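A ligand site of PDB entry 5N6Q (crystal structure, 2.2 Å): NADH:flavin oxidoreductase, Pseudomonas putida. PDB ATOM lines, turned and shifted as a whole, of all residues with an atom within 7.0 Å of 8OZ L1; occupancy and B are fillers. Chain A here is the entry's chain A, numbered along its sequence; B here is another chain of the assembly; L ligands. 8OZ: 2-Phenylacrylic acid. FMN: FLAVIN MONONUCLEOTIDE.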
ATOM      1  N   PRO A  23       9.599   9.204  21.919  1.00  0.00           N
ATOM      2  CA  PRO A  23       8.930   8.904  23.202  1.00  0.00           C
ATOM      3  C   PRO A  23       8.252   7.551  23.156  1.00  0.00           C
ATOM      4  O   PRO A  23       7.534   7.242  22.219  1.00  0.00           O
ATOM      5  CB  PRO A  23       7.908  10.047  23.340  1.00  0.00           C
ATOM      6  CG  PRO A  23       7.697  10.552  21.904  1.00  0.00           C
ATOM      7  CD  PRO A  23       9.054  10.404  21.263  1.00  0.00           C
ATOM      8  N   MET A  24       8.455   6.742  24.210  1.00  0.00           N
ATOM      9  CA  MET A  24       7.836   5.424  24.243  1.00  0.00           C
ATOM     10  C   MET A  24       7.325   5.171  25.645  1.00  0.00           C
ATOM     11  O   MET A  24       8.123   4.955  26.569  1.00  0.00           O
ATOM     12  CB  MET A  24       8.808   4.321  23.804  1.00  0.00           C
ATOM     13  CG  MET A  24       9.148   4.387  22.359  1.00  0.00           C
ATOM     14  SD  MET A  24      10.356   3.144  21.846  1.00  0.00           S
ATOM     15  CE  MET A  24      11.842   3.764  22.603  1.00  0.00           C
ATOM     16  N   CYS A  25       6.000   5.218  25.826  1.00  0.00           N
ATOM     17  CA  CYS A  25       5.438   4.986  27.156  1.00  0.00           C
ATOM     18  C   CYS A  25       5.798   3.600  27.644  1.00  0.00           C
ATOM     19  O   CYS A  25       5.826   2.637  26.876  1.00  0.00           O
ATOM     20  CB  CYS A  25       3.915   5.162  27.188  1.00  0.00           C
ATOM     21  SG  CYS A  25       3.193   4.807  28.868  1.00  0.00           S
ATOM     22  N   TYR A  27       4.335   2.267  30.693  1.00  0.00           N
ATOM     23  CA  TYR A  27       3.220   1.690  31.444  1.00  0.00           C
ATOM     24  C   TYR A  27       3.658   1.238  32.848  1.00  0.00           C
ATOM     25  O   TYR A  27       3.028   0.406  33.485  1.00  0.00           O
ATOM     26  CB  TYR A  27       2.572   0.555  30.646  1.00  0.00           C
ATOM     27  CG  TYR A  27       2.206   1.020  29.244  1.00  0.00           C
ATOM     28  CD1 TYR A  27       1.109   1.862  29.026  1.00  0.00           C
ATOM     29  CD2 TYR A  27       2.985   0.675  28.141  1.00  0.00           C
ATOM     30  CE1 TYR A  27       0.797   2.315  27.759  1.00  0.00           C
ATOM     31  CE2 TYR A  27       2.665   1.119  26.866  1.00  0.00           C
ATOM     32  CZ  TYR A  27       1.574   1.933  26.683  1.00  0.00           C
ATOM     33  OH  TYR A  27       1.271   2.390  25.415  1.00  0.00           O
ATOM     34  N   ALA A  57       5.427   9.947  26.551  1.00  0.00           N
ATOM     35  CA  ALA A  57       4.272  10.809  26.716  1.00  0.00           C
ATOM     36  C   ALA A  57       3.924  11.005  28.193  1.00  0.00           C
ATOM     37  O   ALA A  57       3.555  10.057  28.892  1.00  0.00           O
ATOM     38  CB  ALA A  57       3.089  10.188  25.982  1.00  0.00           C
ATOM     39  N   ILE A  66      -2.871   8.368  28.954  1.00  0.00           N
ATOM     40  CA  ILE A  66      -3.420   7.336  28.085  1.00  0.00           C
ATOM     41  C   ILE A  66      -3.896   6.151  28.915  1.00  0.00           C
ATOM     42  O   ILE A  66      -4.992   5.625  28.702  1.00  0.00           O
ATOM     43  CB  ILE A  66      -2.392   6.878  27.041  1.00  0.00           C
ATOM     44  CG1 ILE A  66      -1.859   8.073  26.268  1.00  0.00           C
ATOM     45  CG2 ILE A  66      -3.035   5.848  26.128  1.00  0.00           C
ATOM     46  CD1 ILE A  66      -0.372   8.033  26.080  1.00  0.00           C
ATOM     47  N   CYS A  70       0.824   5.517  32.869  1.00  0.00           N
ATOM     48  CA  CYS A  70       1.499   6.564  32.148  1.00  0.00           C
ATOM     49  C   CYS A  70       2.116   7.587  33.095  1.00  0.00           C
ATOM     50  O   CYS A  70       1.634   7.799  34.217  1.00  0.00           O
ATOM     51  CB  CYS A  70       0.529   7.254  31.183  1.00  0.00           C
ATOM     52  SG  CYS A  70       0.146   6.196  29.768  1.00  0.00           S
ATOM     53  N   GLN A  99       8.115  14.608  25.996  1.00  0.00           N
ATOM     54  CA  GLN A  99       6.852  14.827  25.306  1.00  0.00           C
ATOM     55  C   GLN A  99       5.766  15.030  26.351  1.00  0.00           C
ATOM     56  O   GLN A  99       5.530  14.160  27.184  1.00  0.00           O
ATOM     57  CB  GLN A  99       6.507  13.638  24.411  1.00  0.00           C
ATOM     58  CG  GLN A  99       5.223  13.795  23.670  1.00  0.00           C
ATOM     59  CD  GLN A  99       4.860  12.515  22.927  1.00  0.00           C
ATOM     60  OE1 GLN A  99       4.539  11.522  23.564  1.00  0.00           O
ATOM     61  NE2 GLN A  99       4.901  12.532  21.593  1.00  0.00           N
ATOM     62  N   LYS A 106      -8.962   9.419  23.750  1.00  0.00           N
ATOM     63  CA  LYS A 106      -8.378   8.078  23.721  1.00  0.00           C
ATOM     64  C   LYS A 106      -7.762   7.632  25.053  1.00  0.00           C
ATOM     65  O   LYS A 106      -7.135   6.571  25.110  1.00  0.00           O
ATOM     66  CB  LYS A 106      -7.357   7.990  22.581  1.00  0.00           C
ATOM     67  CG  LYS A 106      -8.003   8.182  21.198  1.00  0.00           C
ATOM     68  CD  LYS A 106      -6.959   8.291  20.102  1.00  0.00           C
ATOM     69  CE  LYS A 106      -6.478   6.909  19.648  1.00  0.00           C
ATOM     70  NZ  LYS A 106      -5.506   7.049  18.540  1.00  0.00           N
ATOM     71  N   PRO A 112      -1.368  -1.884  27.226  1.00  0.00           N
ATOM     72  CA  PRO A 112      -1.460  -2.717  25.996  1.00  0.00           C
ATOM     73  C   PRO A 112      -1.404  -4.223  26.227  1.00  0.00           C
ATOM     74  O   PRO A 112      -1.985  -4.981  25.438  1.00  0.00           O
ATOM     75  CB  PRO A 112      -0.255  -2.229  25.174  1.00  0.00           C
ATOM     76  CG  PRO A 112      -0.018  -0.837  25.640  1.00  0.00           C
ATOM     77  CD  PRO A 112      -0.374  -0.817  27.098  1.00  0.00           C
ATOM     78  N   ASP A 116      -5.682  -3.437  26.335  1.00  0.00           N
ATOM     79  CA  ASP A 116      -5.432  -2.398  25.336  1.00  0.00           C
ATOM     80  C   ASP A 116      -6.739  -1.727  24.885  1.00  0.00           C
ATOM     81  O   ASP A 116      -6.853  -1.265  23.747  1.00  0.00           O
ATOM     82  CB  ASP A 116      -4.652  -2.973  24.152  1.00  0.00           C
ATOM     83  CG  ASP A 116      -4.016  -1.900  23.281  1.00  0.00           C
ATOM     84  OD1 ASP A 116      -3.080  -1.229  23.786  1.00  0.00           O
ATOM     85  OD2 ASP A 116      -4.423  -1.746  22.109  1.00  0.00           O
ATOM     86  N   HIS A 178       2.567  16.978  22.259  1.00  0.00           N
ATOM     87  CA  HIS A 178       1.975  15.805  21.617  1.00  0.00           C
ATOM     88  C   HIS A 178       0.672  16.203  20.928  1.00  0.00           C
ATOM     89  O   HIS A 178      -0.421  16.052  21.472  1.00  0.00           O
ATOM     90  CB  HIS A 178       1.739  14.689  22.621  1.00  0.00           C
ATOM     91  CG  HIS A 178       1.578  13.333  21.981  1.00  0.00           C
ATOM     92  ND1 HIS A 178       1.460  13.162  20.616  1.00  0.00           N
ATOM     93  CD2 HIS A 178       1.610  12.088  22.521  1.00  0.00           C
ATOM     94  CE1 HIS A 178       1.365  11.866  20.355  1.00  0.00           C
ATOM     95  NE2 HIS A 178       1.467  11.195  21.489  1.00  0.00           N
ATOM     96  N   ALA A 180      -0.269  14.688  18.065  1.00  0.00           N
ATOM     97  CA  ALA A 180      -0.373  13.569  17.133  1.00  0.00           C
ATOM     98  C   ALA A 180      -1.227  12.451  17.733  1.00  0.00           C
ATOM     99  O   ALA A 180      -1.748  12.556  18.856  1.00  0.00           O
ATOM    100  CB  ALA A 180       1.017  13.034  16.765  1.00  0.00           C
ATOM    101  N   HIS A 181      -1.447  11.413  16.905  1.00  0.00           N
ATOM    102  CA  HIS A 181      -1.930  10.075  17.307  1.00  0.00           C
ATOM    103  C   HIS A 181      -3.349  10.106  17.884  1.00  0.00           C
ATOM    104  O   HIS A 181      -3.713   9.241  18.689  1.00  0.00           O
ATOM    105  CB  HIS A 181      -0.970   9.385  18.282  1.00  0.00           C
ATOM    106  CG  HIS A 181       0.407   9.186  17.712  1.00  0.00           C
ATOM    107  ND1 HIS A 181       1.486   8.785  18.477  1.00  0.00           N
ATOM    108  CD2 HIS A 181       0.890   9.368  16.462  1.00  0.00           C
ATOM    109  CE1 HIS A 181       2.561   8.717  17.723  1.00  0.00           C
ATOM    110  NE2 HIS A 181       2.233   9.067  16.490  1.00  0.00           N
ATOM    111  N   GLY A 182      -4.162  11.076  17.461  1.00  0.00           N
ATOM    112  CA  GLY A 182      -5.553  11.125  17.855  1.00  0.00           C
ATOM    113  C   GLY A 182      -5.814  11.660  19.251  1.00  0.00           C
ATOM    114  O   GLY A 182      -6.960  11.625  19.713  1.00  0.00           O
ATOM    115  N   TYR A 183      -4.802  12.204  19.912  1.00  0.00           N
ATOM    116  CA  TYR A 183      -5.053  12.730  21.258  1.00  0.00           C
ATOM    117  C   TYR A 183      -5.646  14.139  21.188  1.00  0.00           C
ATOM    118  O   TYR A 183      -6.155  14.538  20.133  1.00  0.00           O
ATOM    119  CB  TYR A 183      -3.763  12.665  22.046  1.00  0.00           C
ATOM    120  CG  TYR A 183      -3.316  11.241  22.140  1.00  0.00           C
ATOM    121  CD1 TYR A 183      -4.190  10.243  22.560  1.00  0.00           C
ATOM    122  CD2 TYR A 183      -2.036  10.868  21.762  1.00  0.00           C
ATOM    123  CE1 TYR A 183      -3.784   8.904  22.643  1.00  0.00           C
ATOM    124  CE2 TYR A 183      -1.629   9.545  21.826  1.00  0.00           C
ATOM    125  CZ  TYR A 183      -2.500   8.567  22.259  1.00  0.00           C
ATOM    126  OH  TYR A 183      -2.066   7.258  22.320  1.00  0.00           O
ATOM    127  N   ARG A 231       5.016  16.942  17.920  1.00  0.00           N
ATOM    128  CA  ARG A 231       4.717  15.768  17.102  1.00  0.00           C
ATOM    129  C   ARG A 231       3.296  15.937  16.594  1.00  0.00           C
ATOM    130  O   ARG A 231       2.411  16.336  17.360  1.00  0.00           O
ATOM    131  CB  ARG A 231       4.835  14.467  17.899  1.00  0.00           C
ATOM    132  CG  ARG A 231       4.685  13.226  17.041  1.00  0.00           C
ATOM    133  CD  ARG A 231       5.115  11.959  17.780  1.00  0.00           C
ATOM    134  NE  ARG A 231       5.947  11.133  16.918  1.00  0.00           N
ATOM    135  CZ  ARG A 231       6.393   9.925  17.233  1.00  0.00           C
ATOM    136  NH1 ARG A 231       6.086   9.378  18.418  1.00  0.00           N
ATOM    137  NH2 ARG A 231       7.185   9.278  16.372  1.00  0.00           N
ATOM    138  N   PHE A 269      -4.061   8.937  13.367  1.00  0.00           N
ATOM    139  CA  PHE A 269      -4.773   7.919  14.181  1.00  0.00           C
ATOM    140  C   PHE A 269      -6.016   8.494  14.858  1.00  0.00           C
ATOM    141  O   PHE A 269      -6.352   8.113  15.984  1.00  0.00           O
ATOM    142  CB  PHE A 269      -3.842   7.308  15.239  1.00  0.00           C
ATOM    143  CG  PHE A 269      -2.622   6.620  14.678  1.00  0.00           C
ATOM    144  CD1 PHE A 269      -2.732   5.427  13.991  1.00  0.00           C
ATOM    145  CD2 PHE A 269      -1.368   7.177  14.840  1.00  0.00           C
ATOM    146  CE1 PHE A 269      -1.617   4.808  13.475  1.00  0.00           C
ATOM    147  CE2 PHE A 269      -0.249   6.570  14.320  1.00  0.00           C
ATOM    148  CZ  PHE A 269      -0.364   5.389  13.636  1.00  0.00           C
ATOM    149  N   TRP B 358       5.939  -5.432  22.752  1.00  0.00           N
ATOM    150  CA  TRP B 358       6.141  -4.724  21.502  1.00  0.00           C
ATOM    151  C   TRP B 358       7.157  -5.389  20.575  1.00  0.00           C
ATOM    152  O   TRP B 358       7.236  -5.017  19.402  1.00  0.00           O
ATOM    153  CB  TRP B 358       6.569  -3.298  21.819  1.00  0.00           C
ATOM    154  CG  TRP B 358       5.621  -2.693  22.803  1.00  0.00           C
ATOM    155  CD1 TRP B 358       5.791  -2.563  24.160  1.00  0.00           C
ATOM    156  CD2 TRP B 358       4.320  -2.187  22.507  1.00  0.00           C
ATOM    157  NE1 TRP B 358       4.663  -2.000  24.722  1.00  0.00           N
ATOM    158  CE2 TRP B 358       3.746  -1.758  23.728  1.00  0.00           C
ATOM    159  CE3 TRP B 358       3.576  -2.047  21.336  1.00  0.00           C
ATOM    160  CZ2 TRP B 358       2.482  -1.181  23.791  1.00  0.00           C
ATOM    161  CZ3 TRP B 358       2.316  -1.498  21.413  1.00  0.00           C
ATOM    162  CH2 TRP B 358       1.782  -1.061  22.634  1.00  0.00           C
HETATM  163  C4  8OZ L   1       2.146   3.295  20.246  1.00  0.00           C
HETATM  164  C5  8OZ L   1       2.003   2.274  21.172  1.00  0.00           C
HETATM  165  C6  8OZ L   1       1.715   2.562  22.480  1.00  0.00           C
HETATM  166  C7  8OZ L   1       1.555   3.888  22.886  1.00  0.00           C
HETATM  167  C8  8OZ L   1       1.074   7.289  21.279  1.00  0.00           C
HETATM  168  C   8OZ L   1       1.463   6.707  23.647  1.00  0.00           C
HETATM  169  O   8OZ L   1       1.602   8.388  21.183  1.00  0.00           O
HETATM  170  C1  8OZ L   1       1.419   6.328  22.377  1.00  0.00           C
HETATM  171  C2  8OZ L   1       1.680   4.930  21.971  1.00  0.00           C
HETATM  172  C3  8OZ L   1       2.001   4.614  20.647  1.00  0.00           C
HETATM  173  O1  8OZ L   1       0.156   6.858  20.432  1.00  0.00           O
HETATM  174  N1  FMN L   2       4.738   7.684  20.406  1.00  0.00           N
HETATM  175  C2  FMN L   2       4.493   8.845  21.057  1.00  0.00           C
HETATM  176  O2  FMN L   2       4.257   9.893  20.442  1.00  0.00           O
HETATM  177  N3  FMN L   2       4.447   8.849  22.436  1.00  0.00           N
HETATM  178  C4  FMN L   2       4.595   7.749  23.254  1.00  0.00           C
HETATM  179  O4  FMN L   2       4.722   7.888  24.457  1.00  0.00           O
HETATM  180  C4A FMN L   2       4.752   6.528  22.554  1.00  0.00           C
HETATM  181  N5  FMN L   2       4.872   5.439  23.253  1.00  0.00           N
HETATM  182  C5A FMN L   2       5.172   4.275  22.588  1.00  0.00           C
HETATM  183  C6  FMN L   2       5.408   3.143  23.353  1.00  0.00           C
HETATM  184  C7  FMN L   2       5.836   1.958  22.757  1.00  0.00           C
HETATM  185  C7M FMN L   2       6.182   0.781  23.633  1.00  0.00           C
HETATM  186  C8  FMN L   2       5.985   1.899  21.359  1.00  0.00           C
HETATM  187  C8M FMN L   2       6.419   0.635  20.678  1.00  0.00           C
HETATM  188  C9  FMN L   2       5.726   3.034  20.601  1.00  0.00           C
HETATM  189  C9A FMN L   2       5.337   4.228  21.198  1.00  0.00           C
HETATM  190  N10 FMN L   2       5.187   5.423  20.469  1.00  0.00           N
HETATM  191  C10 FMN L   2       4.861   6.590  21.118  1.00  0.00           C
HETATM  192  C1' FMN L   2       5.573   5.490  19.051  1.00  0.00           C
HETATM  193  C2' FMN L   2       7.088   5.635  18.902  1.00  0.00           C
HETATM  194  O2' FMN L   2       7.527   6.924  19.349  1.00  0.00           O
HETATM  195  C3' FMN L   2       7.580   5.451  17.469  1.00  0.00           C
HETATM  196  O3' FMN L   2       7.091   6.519  16.648  1.00  0.00           O
HETATM  197  C4' FMN L   2       7.170   4.127  16.830  1.00  0.00           C
HETATM  198  O4' FMN L   2       7.475   3.068  17.735  1.00  0.00           O
HETATM  199  C5' FMN L   2       7.804   3.914  15.460  1.00  0.00           C
HETATM  200  O5' FMN L   2       9.236   3.815  15.548  1.00  0.00           O
HETATM  201  P   FMN L   2      10.025   2.374  15.645  1.00  0.00           P
HETATM  202  O1P FMN L   2       9.639   1.708  16.920  1.00  0.00           O
HETATM  203  O2P FMN L   2       9.611   1.604  14.381  1.00  0.00           O
HETATM  204  O3P FMN L   2      11.489   2.657  15.525  1.00  0.00           O
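N of Cys 25 lies within hydrogen-bond range of N5 of FMN L2, at 2.8 Å. An oxygen (O3') of FMN L2 sits at hydrogen-bond distance from the guanidinium group of Arg 231 (2.8 Å). A ring nitrogen (ND1) of His 181 sits at hydrogen-bond distance from an oxygen (O) of 8OZ L1. A ring nitrogen (NE2) of His 178 is in hydrogen-bond range of an oxygen (O2) of FMN L2 (3.3 Å). A ring nitrogen (NE2) of His 178 lies within hydrogen-bond range of an oxygen (O) of 8OZ L1. The backbone carbonyl oxygen (O) of Pro 23 sits at hydrogen-bond distance from an oxygen (O2') of FMN L2. OH of Tyr 183 lies within hydrogen-bond range of O1 of 8OZ L1, 2.9 Å away. N of Ala 57 is in hydrogen-bond range of O4 of FMN L2, 3.0 Å away. N3 of FMN L2 sits at hydrogen-bond distance from OE1 of Gln 99, 2.9 Å away.
A nitrogen (N3) of FMN L2 sits close to an oxygen (O) of 8OZ L1.
The backbone NH (N) of Tyr 27 is in hydrogen-bond range of the side-chain sulfur (SG) of Cys 25 (3.3 Å). ND1 of His 178 lies close to N of Ala 180, at 3.4 Å. O of His 181 sits at hydrogen-bond distance from NZ of Lys 106, at 2.8 Å.
Merely in contact with 8OZ L1: Tyr 27 (3.0 Å), Ile 66 (3.3 Å) and Trp 358 of chain B (3.6 Å). Hydrophobic or aromatic side chains that line 8OZ L1: Ile 66, His 178, His 181, Tyr 183 and Trp 358 of chain B. Of the 19 residues printed, 6 come within 4 Å of 8OZ L1. The nearest printed residue that does not touch 8OZ L1 is Ala 57 (4.5 Å).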
